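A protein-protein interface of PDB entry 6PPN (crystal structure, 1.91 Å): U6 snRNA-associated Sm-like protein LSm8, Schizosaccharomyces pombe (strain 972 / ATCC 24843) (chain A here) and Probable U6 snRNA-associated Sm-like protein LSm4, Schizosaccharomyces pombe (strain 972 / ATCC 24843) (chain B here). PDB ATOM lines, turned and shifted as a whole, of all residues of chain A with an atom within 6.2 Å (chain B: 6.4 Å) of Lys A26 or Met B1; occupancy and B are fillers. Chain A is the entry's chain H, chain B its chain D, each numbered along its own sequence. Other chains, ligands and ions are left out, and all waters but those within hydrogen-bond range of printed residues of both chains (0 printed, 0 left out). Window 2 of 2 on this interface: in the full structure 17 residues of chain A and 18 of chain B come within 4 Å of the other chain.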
ATOM      1  N   MET A   7     -10.595  20.260   1.845  1.00  0.00           N
ATOM      2  CA  MET A   7      -9.524  20.781   0.995  1.00  0.00           C
ATOM      3  C   MET A   7      -8.136  20.347   1.473  1.00  0.00           C
ATOM      4  O   MET A   7      -7.846  20.325   2.676  1.00  0.00           O
ATOM      5  CB  MET A   7      -9.590  22.303   0.951  1.00  0.00           C
ATOM      6  CG  MET A   7     -10.611  22.844  -0.019  1.00  0.00           C
ATOM      7  SD  MET A   7     -10.140  22.404  -1.690  1.00  0.00           S
ATOM      8  CE  MET A   7      -8.572  23.262  -1.754  1.00  0.00           C
ATOM      9  N   GLU A   8      -7.270  20.015   0.508  1.00  0.00           N
ATOM     10  CA  GLU A   8      -5.874  19.657   0.743  1.00  0.00           C
ATOM     11  C   GLU A   8      -5.729  18.381   1.557  1.00  0.00           C
ATOM     12  O   GLU A   8      -4.692  18.164   2.191  1.00  0.00           O
ATOM     13  CB  GLU A   8      -5.087  20.786   1.430  1.00  0.00           C
ATOM     14  CG  GLU A   8      -5.215  22.142   0.781  1.00  0.00           C
ATOM     15  CD  GLU A   8      -4.716  22.179  -0.659  1.00  0.00           C
ATOM     16  OE1 GLU A   8      -3.846  21.353  -1.039  1.00  0.00           O
ATOM     17  OE2 GLU A   8      -5.231  23.032  -1.423  1.00  0.00           O
ATOM     18  N   GLN A   9      -6.758  17.544   1.599  1.00  0.00           N
ATOM     19  CA  GLN A   9      -6.671  16.284   2.316  1.00  0.00           C
ATOM     20  C   GLN A   9      -7.001  15.133   1.377  1.00  0.00           C
ATOM     21  O   GLN A   9      -7.591  15.330   0.307  1.00  0.00           O
ATOM     22  CB  GLN A   9      -7.612  16.269   3.526  1.00  0.00           C
ATOM     23  CG  GLN A   9      -7.339  17.404   4.501  1.00  0.00           C
ATOM     24  CD  GLN A   9      -8.555  17.728   5.343  1.00  0.00           C
ATOM     25  OE1 GLN A   9      -8.839  17.053   6.342  1.00  0.00           O
ATOM     26  NE2 GLN A   9      -9.317  18.739   4.911  1.00  0.00           N
ATOM     27  N   SER A  24      -5.734  13.798  -3.374  1.00  0.00           N
ATOM     28  CA  SER A  24      -5.771  15.032  -2.600  1.00  0.00           C
ATOM     29  C   SER A  24      -6.702  16.056  -3.232  1.00  0.00           C
ATOM     30  O   SER A  24      -6.596  16.357  -4.427  1.00  0.00           O
ATOM     31  CB  SER A  24      -4.369  15.591  -2.467  1.00  0.00           C
ATOM     32  OG  SER A  24      -3.550  14.586  -1.909  1.00  0.00           O
ATOM     33  N   LEU A  25      -7.627  16.594  -2.439  1.00  0.00           N
ATOM     34  CA  LEU A  25      -8.586  17.540  -3.002  1.00  0.00           C
ATOM     35  C   LEU A  25      -7.878  18.873  -3.161  1.00  0.00           C
ATOM     36  O   LEU A  25      -7.473  19.494  -2.171  1.00  0.00           O
ATOM     37  CB  LEU A  25      -9.828  17.664  -2.125  1.00  0.00           C
ATOM     38  CG  LEU A  25     -10.949  18.576  -2.649  1.00  0.00           C
ATOM     39  CD1 LEU A  25     -11.472  18.033  -3.979  1.00  0.00           C
ATOM     40  CD2 LEU A  25     -12.097  18.667  -1.666  1.00  0.00           C
ATOM     41  N   LYS A  26      -7.687  19.295  -4.407  1.00  0.00           N
ATOM     42  CA  LYS A  26      -7.039  20.569  -4.662  1.00  0.00           C
ATOM     43  C   LYS A  26      -8.037  21.658  -5.013  1.00  0.00           C
ATOM     44  O   LYS A  26      -7.690  22.838  -4.961  1.00  0.00           O
ATOM     45  CB  LYS A  26      -6.003  20.423  -5.789  1.00  0.00           C
ATOM     46  CG  LYS A  26      -5.046  19.259  -5.576  1.00  0.00           C
ATOM     47  CD  LYS A  26      -4.128  19.414  -4.359  1.00  0.00           C
ATOM     48  CE  LYS A  26      -3.123  20.517  -4.494  1.00  0.00           C
ATOM     49  NZ  LYS A  26      -2.295  20.673  -3.230  1.00  0.00           N
ATOM     50  N   GLY A  27      -9.272  21.311  -5.334  1.00  0.00           N
ATOM     51  CA  GLY A  27     -10.210  22.394  -5.542  1.00  0.00           C
ATOM     52  C   GLY A  27     -11.534  21.860  -6.019  1.00  0.00           C
ATOM     53  O   GLY A  27     -11.592  20.716  -6.451  1.00  0.00           O
ATOM     54  N   PHE A  28     -12.593  22.669  -5.938  1.00  0.00           N
ATOM     55  CA  PHE A  28     -13.911  22.277  -6.388  1.00  0.00           C
ATOM     56  C   PHE A  28     -14.663  23.540  -6.783  1.00  0.00           C
ATOM     57  O   PHE A  28     -14.234  24.659  -6.492  1.00  0.00           O
ATOM     58  CB  PHE A  28     -14.657  21.540  -5.279  1.00  0.00           C
ATOM     59  CG  PHE A  28     -14.896  22.379  -4.071  1.00  0.00           C
ATOM     60  CD1 PHE A  28     -13.911  22.520  -3.111  1.00  0.00           C
ATOM     61  CD2 PHE A  28     -16.097  23.041  -3.897  1.00  0.00           C
ATOM     62  CE1 PHE A  28     -14.120  23.307  -1.991  1.00  0.00           C
ATOM     63  CE2 PHE A  28     -16.320  23.829  -2.797  1.00  0.00           C
ATOM     64  CZ  PHE A  28     -15.325  23.968  -1.822  1.00  0.00           C
ATOM     65  N   ILE A  35     -10.848  18.758  -8.486  1.00  0.00           N
ATOM     66  CA  ILE A  35      -9.470  18.454  -8.856  1.00  0.00           C
ATOM     67  C   ILE A  35      -8.905  17.526  -7.790  1.00  0.00           C
ATOM     68  O   ILE A  35      -8.814  17.908  -6.617  1.00  0.00           O
ATOM     69  CB  ILE A  35      -8.595  19.715  -8.940  1.00  0.00           C
ATOM     70  CG1 ILE A  35      -9.152  20.741  -9.917  1.00  0.00           C
ATOM     71  CG2 ILE A  35      -7.166  19.330  -9.344  1.00  0.00           C
ATOM     72  CD1 ILE A  35      -8.491  22.125  -9.747  1.00  0.00           C
ATOM     73  N   LEU A  36      -8.423  16.361  -8.204  1.00  0.00           N
ATOM     74  CA  LEU A  36      -7.656  15.480  -7.336  1.00  0.00           C
ATOM     75  C   LEU A  36      -6.237  15.378  -7.876  1.00  0.00           C
ATOM     76  O   LEU A  36      -6.037  15.273  -9.086  1.00  0.00           O
ATOM     77  CB  LEU A  36      -8.263  14.085  -7.294  1.00  0.00           C
ATOM     78  CG  LEU A  36      -9.736  14.013  -6.952  1.00  0.00           C
ATOM     79  CD1 LEU A  36     -10.136  12.560  -6.794  1.00  0.00           C
ATOM     80  CD2 LEU A  36      -9.964  14.765  -5.717  1.00  0.00           C
ATOM     81  N   SER A  37      -5.245  15.431  -6.994  1.00  0.00           N
ATOM     82  CA  SER A  37      -3.869  15.200  -7.408  1.00  0.00           C
ATOM     83  C   SER A  37      -3.309  13.996  -6.672  1.00  0.00           C
ATOM     84  O   SER A  37      -3.857  13.567  -5.654  1.00  0.00           O
ATOM     85  CB  SER A  37      -2.999  16.427  -7.161  1.00  0.00           C
ATOM     86  OG  SER A  37      -2.901  16.686  -5.782  1.00  0.00           O
ATOM     87  N   MET B   1      -8.123  25.922  -5.561  1.00  0.00           N
ATOM     88  CA  MET B   1      -7.923  26.153  -6.985  1.00  0.00           C
ATOM     89  C   MET B   1      -9.177  25.765  -7.769  1.00  0.00           C
ATOM     90  O   MET B   1      -9.701  24.665  -7.589  1.00  0.00           O
ATOM     91  CB  MET B   1      -6.710  25.366  -7.471  1.00  0.00           C
ATOM     92  CG  MET B   1      -6.671  25.225  -8.977  1.00  0.00           C
ATOM     93  SD  MET B   1      -5.151  24.591  -9.681  1.00  0.00           S
ATOM     94  CE  MET B   1      -3.927  25.068  -8.443  1.00  0.00           C
ATOM     95  N   LEU B   2      -9.651  26.648  -8.675  1.00  0.00           N
ATOM     96  CA  LEU B   2     -10.892  26.255  -9.342  1.00  0.00           C
ATOM     97  C   LEU B   2     -10.613  25.292 -10.492  1.00  0.00           C
ATOM     98  O   LEU B   2      -9.620  25.459 -11.210  1.00  0.00           O
ATOM     99  CB  LEU B   2     -11.620  27.483  -9.876  1.00  0.00           C
ATOM    100  CG  LEU B   2     -12.248  28.383  -8.827  1.00  0.00           C
ATOM    101  CD1 LEU B   2     -12.533  29.727  -9.398  1.00  0.00           C
ATOM    102  CD2 LEU B   2     -13.540  27.745  -8.345  1.00  0.00           C
ATOM    103  N   PRO B   3     -11.496  24.302 -10.700  1.00  0.00           N
ATOM    104  CA  PRO B   3     -11.287  23.332 -11.793  1.00  0.00           C
ATOM    105  C   PRO B   3     -11.182  23.979 -13.161  1.00  0.00           C
ATOM    106  O   PRO B   3     -10.332  23.584 -13.968  1.00  0.00           O
ATOM    107  CB  PRO B   3     -12.529  22.429 -11.696  1.00  0.00           C
ATOM    108  CG  PRO B   3     -12.930  22.494 -10.259  1.00  0.00           C
ATOM    109  CD  PRO B   3     -12.603  23.918  -9.812  1.00  0.00           C
ATOM    110  N   LEU B   4     -11.990  25.006 -13.438  1.00  0.00           N
ATOM    111  CA  LEU B   4     -11.870  25.642 -14.749  1.00  0.00           C
ATOM    112  C   LEU B   4     -10.590  26.457 -14.847  1.00  0.00           C
ATOM    113  O   LEU B   4     -10.047  26.640 -15.944  1.00  0.00           O
ATOM    114  CB  LEU B   4     -13.073  26.520 -15.054  1.00  0.00           C
ATOM    115  CG  LEU B   4     -14.381  25.837 -15.411  1.00  0.00           C
ATOM    116  CD1 LEU B   4     -15.286  26.905 -15.965  1.00  0.00           C
ATOM    117  CD2 LEU B   4     -14.200  24.713 -16.411  1.00  0.00           C
ATOM    118  N   THR B   5     -10.066  26.941 -13.725  1.00  0.00           N
ATOM    119  CA  THR B   5      -8.766  27.579 -13.814  1.00  0.00           C
ATOM    120  C   THR B   5      -7.709  26.567 -14.254  1.00  0.00           C
ATOM    121  O   THR B   5      -6.917  26.839 -15.160  1.00  0.00           O
ATOM    122  CB  THR B   5      -8.416  28.206 -12.478  1.00  0.00           C
ATOM    123  OG1 THR B   5      -9.398  29.196 -12.165  1.00  0.00           O
ATOM    124  CG2 THR B   5      -7.051  28.895 -12.540  1.00  0.00           C
ATOM    125  N   LEU B   6      -7.743  25.359 -13.695  1.00  0.00           N
ATOM    126  CA  LEU B   6      -6.798  24.335 -14.133  1.00  0.00           C
ATOM    127  C   LEU B   6      -7.011  23.976 -15.597  1.00  0.00           C
ATOM    128  O   LEU B   6      -6.054  23.880 -16.380  1.00  0.00           O
ATOM    129  CB  LEU B   6      -6.972  23.084 -13.270  1.00  0.00           C
ATOM    130  CG  LEU B   6      -5.806  22.127 -12.986  1.00  0.00           C
ATOM    131  CD1 LEU B   6      -6.253  20.675 -13.036  1.00  0.00           C
ATOM    132  CD2 LEU B   6      -4.627  22.375 -13.859  1.00  0.00           C
ATOM    133  N   VAL B  75       1.165  21.041 -15.086  1.00  0.00           N
ATOM    134  CA  VAL B  75       0.147  22.081 -15.186  1.00  0.00           C
ATOM    135  C   VAL B  75      -0.336  22.484 -13.802  1.00  0.00           C
ATOM    136  O   VAL B  75      -0.425  23.676 -13.475  1.00  0.00           O
ATOM    137  CB  VAL B  75      -1.015  21.612 -16.060  1.00  0.00           C
ATOM    138  CG1 VAL B  75      -1.981  22.754 -16.217  1.00  0.00           C
ATOM    139  CG2 VAL B  75      -0.470  21.182 -17.403  1.00  0.00           C
ATOM    140  N   LEU B  76      -0.676  21.492 -12.974  1.00  0.00           N
ATOM    141  CA  LEU B  76      -1.119  21.804 -11.620  1.00  0.00           C
ATOM    142  C   LEU B  76      -0.038  22.545 -10.870  1.00  0.00           C
ATOM    143  O   LEU B  76      -0.319  23.529 -10.171  1.00  0.00           O
ATOM    144  CB  LEU B  76      -1.522  20.532 -10.878  1.00  0.00           C
ATOM    145  CG  LEU B  76      -2.011  20.750  -9.441  1.00  0.00           C
ATOM    146  CD1 LEU B  76      -3.315  21.557  -9.344  1.00  0.00           C
ATOM    147  CD2 LEU B  76      -2.183  19.403  -8.776  1.00  0.00           C
ATOM    148  N   VAL B  79       0.102  26.235 -12.063  1.00  0.00           N
ATOM    149  CA  VAL B  79      -0.972  27.080 -11.553  1.00  0.00           C
ATOM    150  C   VAL B  79      -0.760  27.391 -10.076  1.00  0.00           C
ATOM    151  O   VAL B  79      -0.909  28.546  -9.645  1.00  0.00           O
ATOM    152  CB  VAL B  79      -2.323  26.412 -11.800  1.00  0.00           C
ATOM    153  CG1 VAL B  79      -3.446  27.308 -11.329  1.00  0.00           C
ATOM    154  CG2 VAL B  79      -2.468  26.131 -13.253  1.00  0.00           C
ATOM    155  N   ALA B  80      -0.380  26.384  -9.281  1.00  0.00           N
ATOM    156  CA  ALA B  80      -0.131  26.652  -7.868  1.00  0.00           C
ATOM    157  C   ALA B  80       0.992  27.662  -7.688  1.00  0.00           C
ATOM    158  O   ALA B  80       0.896  28.564  -6.844  1.00  0.00           O
ATOM    159  CB  ALA B  80       0.185  25.356  -7.130  1.00  0.00           C
ATOM    160  N   GLN B  83      -0.352  31.168  -8.533  1.00  0.00           N
ATOM    161  CA  GLN B  83      -1.276  31.704  -7.541  1.00  0.00           C
ATOM    162  C   GLN B  83      -0.562  32.049  -6.246  1.00  0.00           C
ATOM    163  O   GLN B  83      -0.924  33.024  -5.576  1.00  0.00           O
ATOM    164  CB  GLN B  83      -2.388  30.703  -7.247  1.00  0.00           C
ATOM    165  CG  GLN B  83      -3.336  30.450  -8.383  1.00  0.00           C
ATOM    166  CD  GLN B  83      -4.435  29.507  -7.973  1.00  0.00           C
ATOM    167  OE1 GLN B  83      -4.306  28.795  -6.967  1.00  0.00           O
ATOM    168  NE2 GLN B  83      -5.532  29.497  -8.731  1.00  0.00           N
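The side-chain carboxylate (OE1) of Glu A8 lies within salt-bridge range of the side-chain amino group (NZ) of Lys A26 (2.8 Å). O of Ser A37 sits at hydrogen-bond distance from N of Ser A24 (3.0 Å). The backbone carbonyl oxygen of Ile A35 is in hydrogen-bond range of the backbone NH of Lys A26, 2.8 Å away. O of Gly A27 sits at hydrogen-bond distance from N of Ile A35 (2.9 Å).
Lys A26 touches just one residue of chain B: Met B1 (3.2 Å). Met B1 touches four residues of chain A. Of the printed residues of chain B, Gly A27 touches Met B1 (3.1 Å). Of the printed residues of chain B, Ser A37 touches Leu B76. Of the printed residues of chain B, Phe A28 touches Met B1, Leu B2 and Pro B3. Printed residues of chain A within 4 Å of Leu B2: Phe A28 and Ile A35. The nearest residue of chain B that does not touch Lys A26 is Leu B76 (4.3 Å). The nearest printed residue of chain B that does not touch Phe A28 is Leu B4 (7.3 Å).
Hydrophobic or aromatic side chains of chain B that line the printed part of chain A: Met B1, Leu B2, Pro B3, Leu B6 and Leu B76. Hydrophobic or aromatic side chains of chain A that line the printed part of chain B: Ile A35. Among the printed residues, 10 pairs touch across the chains. Among the printed residues, no Asp or Glu carboxylate lies within 4 Å of a Lys or Arg side-chain nitrogen of the other chain.
O of Lys A26 sits at hydrogen-bond distance from N of Met B1 (3.2 Å).
Among the printed residues, merely in contact across the chains: Gly A27 with Met B1 (3.1 Å), Phe A28 with Met B1 (3.9 Å), Phe A28 with Leu B2 (3.7 Å), Phe A28 with Pro B3 (3.7 Å), Ile A35 with Met B1 (3.5 Å), Ile A35 with Leu B2 (3.8 Å), Ile A35 with Pro B3 (3.7 Å), Ile A35 with Leu B6 (3.95 Å) and Ser A37 with Leu B76 (3.5 Å).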
